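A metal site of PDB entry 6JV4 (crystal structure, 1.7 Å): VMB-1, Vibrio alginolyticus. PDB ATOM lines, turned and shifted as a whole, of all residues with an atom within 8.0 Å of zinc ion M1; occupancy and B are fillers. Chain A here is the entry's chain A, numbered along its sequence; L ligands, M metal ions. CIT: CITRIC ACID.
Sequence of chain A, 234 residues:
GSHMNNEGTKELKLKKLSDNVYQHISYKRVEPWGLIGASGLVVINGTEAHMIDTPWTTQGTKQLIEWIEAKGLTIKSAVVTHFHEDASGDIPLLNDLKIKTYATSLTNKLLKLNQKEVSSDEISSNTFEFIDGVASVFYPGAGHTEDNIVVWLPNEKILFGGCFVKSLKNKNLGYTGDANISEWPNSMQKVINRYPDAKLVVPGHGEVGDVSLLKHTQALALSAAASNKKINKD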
ATOM      1  N   TRP A  56     -24.985 -17.206  -9.326  1.00  0.00           N
ATOM      2  CA  TRP A  56     -24.840 -15.792  -9.772  1.00  0.00           C
ATOM      3  C   TRP A  56     -25.182 -14.779  -8.675  1.00  0.00           C
ATOM      4  O   TRP A  56     -24.763 -13.630  -8.794  1.00  0.00           O
ATOM      5  CB  TRP A  56     -25.681 -15.618 -11.020  1.00  0.00           C
ATOM      6  CG  TRP A  56     -25.197 -14.591 -11.975  1.00  0.00           C
ATOM      7  CD1 TRP A  56     -24.266 -13.608 -11.817  1.00  0.00           C
ATOM      8  CD2 TRP A  56     -25.688 -14.478 -13.316  1.00  0.00           C
ATOM      9  NE1 TRP A  56     -24.127 -12.911 -12.991  1.00  0.00           N
ATOM     10  CE2 TRP A  56     -24.988 -13.421 -13.912  1.00  0.00           C
ATOM     11  CE3 TRP A  56     -26.642 -15.182 -14.036  1.00  0.00           C
ATOM     12  CZ2 TRP A  56     -25.215 -13.055 -15.229  1.00  0.00           C
ATOM     13  CZ3 TRP A  56     -26.876 -14.798 -15.343  1.00  0.00           C
ATOM     14  CH2 TRP A  56     -26.143 -13.772 -15.918  1.00  0.00           C
ATOM     15  N   HIS A  82     -14.328 -18.772 -15.516  1.00  0.00           N
ATOM     16  CA  HIS A  82     -13.783 -17.530 -16.111  1.00  0.00           C
ATOM     17  C   HIS A  82     -13.986 -16.361 -15.147  1.00  0.00           C
ATOM     18  O   HIS A  82     -14.539 -16.586 -14.091  1.00  0.00           O
ATOM     19  CB  HIS A  82     -14.285 -17.218 -17.504  1.00  0.00           C
ATOM     20  CG  HIS A  82     -15.685 -16.761 -17.648  1.00  0.00           C
ATOM     21  ND1 HIS A  82     -16.737 -17.606 -17.464  1.00  0.00           N
ATOM     22  CD2 HIS A  82     -16.199 -15.567 -18.052  1.00  0.00           C
ATOM     23  CE1 HIS A  82     -17.872 -16.954 -17.751  1.00  0.00           C
ATOM     24  NE2 HIS A  82     -17.553 -15.693 -18.058  1.00  0.00           N
ATOM     25  N   PHE A  83     -13.382 -15.215 -15.468  1.00  0.00           N
ATOM     26  CA  PHE A  83     -13.271 -14.125 -14.473  1.00  0.00           C
ATOM     27  C   PHE A  83     -14.584 -13.354 -14.299  1.00  0.00           C
ATOM     28  O   PHE A  83     -14.654 -12.574 -13.324  1.00  0.00           O
ATOM     29  CB  PHE A  83     -12.124 -13.180 -14.835  1.00  0.00           C
ATOM     30  CG  PHE A  83     -12.416 -12.182 -15.924  1.00  0.00           C
ATOM     31  CD1 PHE A  83     -12.381 -12.572 -17.245  1.00  0.00           C
ATOM     32  CD2 PHE A  83     -12.703 -10.854 -15.618  1.00  0.00           C
ATOM     33  CE1 PHE A  83     -12.603 -11.652 -18.266  1.00  0.00           C
ATOM     34  CE2 PHE A  83     -12.938  -9.954 -16.640  1.00  0.00           C
ATOM     35  CZ  PHE A  83     -12.838 -10.333 -17.946  1.00  0.00           C
ATOM     36  N   HIS A  84     -15.572 -13.510 -15.193  1.00  0.00           N
ATOM     37  CA  HIS A  84     -16.854 -12.770 -15.077  1.00  0.00           C
ATOM     38  C   HIS A  84     -17.605 -13.197 -13.802  1.00  0.00           C
ATOM     39  O   HIS A  84     -17.448 -14.322 -13.296  1.00  0.00           O
ATOM     40  CB  HIS A  84     -17.724 -12.930 -16.331  1.00  0.00           C
ATOM     41  CG  HIS A  84     -17.218 -12.260 -17.551  1.00  0.00           C
ATOM     42  ND1 HIS A  84     -17.647 -12.631 -18.800  1.00  0.00           N
ATOM     43  CD2 HIS A  84     -16.327 -11.269 -17.748  1.00  0.00           C
ATOM     44  CE1 HIS A  84     -17.070 -11.869 -19.715  1.00  0.00           C
ATOM     45  NE2 HIS A  84     -16.250 -11.007 -19.087  1.00  0.00           N
ATOM     46  N   GLU A  85     -18.563 -12.368 -13.346  1.00  0.00           N
ATOM     47  CA  GLU A  85     -19.317 -12.559 -12.096  1.00  0.00           C
ATOM     48  C   GLU A  85     -20.235 -13.780 -12.143  1.00  0.00           C
ATOM     49  O   GLU A  85     -20.451 -14.372 -11.090  1.00  0.00           O
ATOM     50  CB  GLU A  85     -20.172 -11.305 -11.818  1.00  0.00           C
ATOM     51  CG  GLU A  85     -20.894 -11.333 -10.500  1.00  0.00           C
ATOM     52  CD  GLU A  85     -22.032 -10.320 -10.401  1.00  0.00           C
ATOM     53  OE1 GLU A  85     -22.116  -9.432 -11.292  1.00  0.00           O
ATOM     54  OE2 GLU A  85     -22.805 -10.429  -9.461  1.00  0.00           O
ATOM     55  N   ASP A  86     -20.742 -14.199 -13.295  1.00  0.00           N
ATOM     56  CA  ASP A  86     -21.594 -15.419 -13.328  1.00  0.00           C
ATOM     57  C   ASP A  86     -20.797 -16.692 -12.983  1.00  0.00           C
ATOM     58  O   ASP A  86     -21.408 -17.735 -12.677  1.00  0.00           O
ATOM     59  CB  ASP A  86     -22.344 -15.574 -14.653  1.00  0.00           C
ATOM     60  CG  ASP A  86     -21.506 -15.654 -15.885  1.00  0.00           C
ATOM     61  OD1 ASP A  86     -20.311 -15.244 -15.865  1.00  0.00           O
ATOM     62  OD2 ASP A  86     -22.070 -16.102 -16.919  1.00  0.00           O
ATOM     63  N   ALA A  87     -19.470 -16.673 -13.161  1.00  0.00           N
ATOM     64  CA  ALA A  87     -18.615 -17.844 -12.881  1.00  0.00           C
ATOM     65  C   ALA A  87     -17.929 -17.674 -11.540  1.00  0.00           C
ATOM     66  O   ALA A  87     -17.788 -18.683 -10.858  1.00  0.00           O
ATOM     67  CB  ALA A  87     -17.643 -18.054 -14.003  1.00  0.00           C
ATOM     68  N   HIS A 144     -15.002 -17.046 -25.412  1.00  0.00           N
ATOM     69  CA  HIS A 144     -15.882 -16.098 -24.692  1.00  0.00           C
ATOM     70  C   HIS A 144     -15.023 -15.070 -23.938  1.00  0.00           C
ATOM     71  O   HIS A 144     -15.392 -13.857 -23.925  1.00  0.00           O
ATOM     72  CB  HIS A 144     -16.792 -16.877 -23.775  1.00  0.00           C
ATOM     73  CG  HIS A 144     -17.534 -16.005 -22.829  1.00  0.00           C
ATOM     74  ND1 HIS A 144     -18.534 -15.165 -23.258  1.00  0.00           N
ATOM     75  CD2 HIS A 144     -17.380 -15.779 -21.502  1.00  0.00           C
ATOM     76  CE1 HIS A 144     -19.019 -14.539 -22.189  1.00  0.00           C
ATOM     77  NE2 HIS A 144     -18.359 -14.888 -21.130  1.00  0.00           N
ATOM     78  N   THR A 145     -13.954 -15.531 -23.309  1.00  0.00           N
ATOM     79  CA  THR A 145     -12.947 -14.681 -22.675  1.00  0.00           C
ATOM     80  C   THR A 145     -11.573 -15.289 -22.979  1.00  0.00           C
ATOM     81  O   THR A 145     -11.481 -16.422 -23.444  1.00  0.00           O
ATOM     82  CB  THR A 145     -13.169 -14.508 -21.167  1.00  0.00           C
ATOM     83  OG1 THR A 145     -13.160 -15.836 -20.635  1.00  0.00           O
ATOM     84  CG2 THR A 145     -14.436 -13.793 -20.798  1.00  0.00           C
ATOM     85  N   ASP A 147      -9.532 -16.240 -20.743  1.00  0.00           N
ATOM     86  CA  ASP A 147      -9.194 -17.184 -19.659  1.00  0.00           C
ATOM     87  C   ASP A 147     -10.105 -18.411 -19.586  1.00  0.00           C
ATOM     88  O   ASP A 147      -9.822 -19.290 -18.768  1.00  0.00           O
ATOM     89  CB  ASP A 147      -9.196 -16.474 -18.307  1.00  0.00           C
ATOM     90  CG  ASP A 147     -10.560 -15.924 -17.941  1.00  0.00           C
ATOM     91  OD1 ASP A 147     -11.215 -15.395 -18.847  1.00  0.00           O
ATOM     92  OD2 ASP A 147     -10.922 -16.044 -16.778  1.00  0.00           O
ATOM     93  N   ASN A 148     -11.156 -18.503 -20.378  1.00  0.00           N
ATOM     94  CA  ASN A 148     -12.222 -19.507 -20.155  1.00  0.00           C
ATOM     95  C   ASN A 148     -11.630 -20.935 -20.144  1.00  0.00           C
ATOM     96  O   ASN A 148     -10.803 -21.264 -21.041  1.00  0.00           O
ATOM     97  CB  ASN A 148     -13.390 -19.353 -21.151  1.00  0.00           C
ATOM     98  CG  ASN A 148     -13.036 -19.293 -22.615  1.00  0.00           C
ATOM     99  OD1 ASN A 148     -11.956 -19.813 -23.073  1.00  0.00           O
ATOM    100  ND2 ASN A 148     -13.888 -18.644 -23.360  1.00  0.00           N
ATOM    101  N   GLY A 162     -19.211 -24.087 -19.617  1.00  0.00           N
ATOM    102  CA  GLY A 162     -19.281 -22.713 -19.130  1.00  0.00           C
ATOM    103  C   GLY A 162     -19.608 -21.755 -20.241  1.00  0.00           C
ATOM    104  O   GLY A 162     -20.217 -22.165 -21.280  1.00  0.00           O
ATOM    105  N   CYS A 163     -19.211 -20.500 -20.113  1.00  0.00           N
ATOM    106  CA  CYS A 163     -19.642 -19.503 -21.106  1.00  0.00           C
ATOM    107  C   CYS A 163     -18.906 -19.604 -22.436  1.00  0.00           C
ATOM    108  O   CYS A 163     -19.318 -18.946 -23.384  1.00  0.00           O
ATOM    109  CB  CYS A 163     -19.580 -18.107 -20.510  1.00  0.00           C
ATOM    110  SG  CYS A 163     -20.830 -18.009 -19.191  1.00  0.00           S
ATOM    111  N   PHE A 164     -17.871 -20.451 -22.523  1.00  0.00           N
ATOM    112  CA  PHE A 164     -17.230 -20.840 -23.787  1.00  0.00           C
ATOM    113  C   PHE A 164     -18.186 -21.609 -24.688  1.00  0.00           C
ATOM    114  O   PHE A 164     -17.887 -21.662 -25.945  1.00  0.00           O
ATOM    115  CB  PHE A 164     -16.042 -21.722 -23.422  1.00  0.00           C
ATOM    116  CG  PHE A 164     -15.179 -22.212 -24.539  1.00  0.00           C
ATOM    117  CD1 PHE A 164     -14.325 -21.339 -25.200  1.00  0.00           C
ATOM    118  CD2 PHE A 164     -15.175 -23.557 -24.893  1.00  0.00           C
ATOM    119  CE1 PHE A 164     -13.503 -21.785 -26.213  1.00  0.00           C
ATOM    120  CE2 PHE A 164     -14.403 -23.977 -25.954  1.00  0.00           C
ATOM    121  CZ  PHE A 164     -13.531 -23.108 -26.588  1.00  0.00           C
ATOM    122  N   LYS A 166     -22.149 -22.069 -26.036  1.00  0.00           N
ATOM    123  CA  LYS A 166     -23.519 -21.508 -26.113  1.00  0.00           C
ATOM    124  C   LYS A 166     -24.521 -22.660 -26.177  1.00  0.00           C
ATOM    125  O   LYS A 166     -24.179 -23.782 -26.569  1.00  0.00           O
ATOM    126  CB  LYS A 166     -23.651 -20.622 -27.365  1.00  0.00           C
ATOM    127  CG  LYS A 166     -22.602 -19.522 -27.494  1.00  0.00           C
ATOM    128  CD  LYS A 166     -22.527 -18.605 -26.288  1.00  0.00           C
ATOM    129  CE  LYS A 166     -23.737 -17.723 -26.075  1.00  0.00           C
ATOM    130  NZ  LYS A 166     -23.499 -16.744 -24.974  1.00  0.00           N
ATOM    131  N   TYR A 175     -22.489 -11.839 -24.854  1.00  0.00           N
ATOM    132  CA  TYR A 175     -21.602 -10.706 -24.549  1.00  0.00           C
ATOM    133  C   TYR A 175     -20.207 -10.973 -25.111  1.00  0.00           C
ATOM    134  O   TYR A 175     -19.533 -11.951 -24.683  1.00  0.00           O
ATOM    135  CB  TYR A 175     -21.502 -10.455 -23.055  1.00  0.00           C
ATOM    136  CG  TYR A 175     -20.531  -9.361 -22.730  1.00  0.00           C
ATOM    137  CD1 TYR A 175     -20.774  -8.072 -23.145  1.00  0.00           C
ATOM    138  CD2 TYR A 175     -19.342  -9.620 -22.059  1.00  0.00           C
ATOM    139  CE1 TYR A 175     -19.904  -7.055 -22.811  1.00  0.00           C
ATOM    140  CE2 TYR A 175     -18.457  -8.622 -21.729  1.00  0.00           C
ATOM    141  CZ  TYR A 175     -18.745  -7.322 -22.088  1.00  0.00           C
ATOM    142  OH  TYR A 175     -17.866  -6.317 -21.814  1.00  0.00           O
ATOM    143  N   ASP A 178     -15.319  -9.029 -24.012  1.00  0.00           N
ATOM    144  CA  ASP A 178     -14.050  -9.606 -23.566  1.00  0.00           C
ATOM    145  C   ASP A 178     -13.699 -10.837 -24.398  1.00  0.00           C
ATOM    146  O   ASP A 178     -12.699 -11.521 -24.070  1.00  0.00           O
ATOM    147  CB  ASP A 178     -14.110  -9.978 -22.078  1.00  0.00           C
ATOM    148  CG  ASP A 178     -14.268  -8.747 -21.183  1.00  0.00           C
ATOM    149  OD1 ASP A 178     -13.550  -7.772 -21.469  1.00  0.00           O
ATOM    150  OD2 ASP A 178     -15.049  -8.817 -20.230  1.00  0.00           O
ATOM    151  N   HIS A 205     -25.029 -20.666 -20.087  1.00  0.00           N
ATOM    152  CA  HIS A 205     -26.426 -20.174 -20.120  1.00  0.00           C
ATOM    153  C   HIS A 205     -27.273 -21.098 -20.961  1.00  0.00           C
ATOM    154  O   HIS A 205     -26.772 -21.631 -21.962  1.00  0.00           O
ATOM    155  CB  HIS A 205     -26.509 -18.735 -20.678  1.00  0.00           C
ATOM    156  CG  HIS A 205     -25.580 -17.815 -19.991  1.00  0.00           C
ATOM    157  ND1 HIS A 205     -25.766 -17.430 -18.688  1.00  0.00           N
ATOM    158  CD2 HIS A 205     -24.416 -17.242 -20.355  1.00  0.00           C
ATOM    159  CE1 HIS A 205     -24.762 -16.692 -18.271  1.00  0.00           C
ATOM    160  NE2 HIS A 205     -23.931 -16.574 -19.253  1.00  0.00           N
HETATM  161  C1  CIT L   1     -22.262 -11.185 -17.666  1.00  0.00           C
HETATM  162  O1  CIT L   1     -22.393  -9.996 -17.326  1.00  0.00           O
HETATM  163  O2  CIT L   1     -21.816 -12.076 -16.927  1.00  0.00           O
HETATM  164  C2  CIT L   1     -22.692 -11.575 -19.075  1.00  0.00           C
HETATM  165  C3  CIT L   1     -22.516 -13.053 -19.431  1.00  0.00           C
HETATM  166  O7  CIT L   1     -23.109 -13.859 -18.434  1.00  0.00           O
HETATM  167  C4  CIT L   1     -23.204 -13.323 -20.779  1.00  0.00           C
HETATM  168  C5  CIT L   1     -22.590 -14.440 -21.613  1.00  0.00           C
HETATM  169  O3  CIT L   1     -22.628 -14.329 -22.851  1.00  0.00           O
HETATM  170  O4  CIT L   1     -22.071 -15.397 -21.020  1.00  0.00           O
HETATM  171  C6  CIT L   1     -21.004 -13.378 -19.548  1.00  0.00           C
HETATM  172  O5  CIT L   1     -20.282 -12.560 -20.156  1.00  0.00           O
HETATM  173  O6  CIT L   1     -20.607 -14.441 -19.034  1.00  0.00           O
HETATM  174 ZN    ZN M   1     -18.676 -14.292 -19.209  1.00  0.00          ZN
HETATM  175 ZN    ZN M   2     -21.930 -15.949 -18.977  1.00  0.00          ZN
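Zinc ion M1 is bound by an oxygen (O6) of the ligand (1.9 Å), a ring nitrogen (ND1) of His 84 (2.0 Å), a ring nitrogen (NE2) of His 144 (2.0 Å), a ring nitrogen (NE2) of His 82 (2.1 Å) and an oxygen (O5) of the ligand (2.5 Å).
The side-chain amide nitrogen (ND2) of Asn 148 sits close to the backbone NH (N) of His 144 (2.8 Å). The side-chain carboxylate (OD2) of Asp 178 lies within hydrogen-bond range of a ring nitrogen (NE2) of His 84, 2.7 Å away.
Merely in contact with zinc ion M1: Asp 86 (3.8 Å). Within 4 Å of zinc ion M1: His 82, His 84, Asp 86 and His 144. The nearest printed residue that does not touch zinc ion M1 is Cys 163 (4.1 Å).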
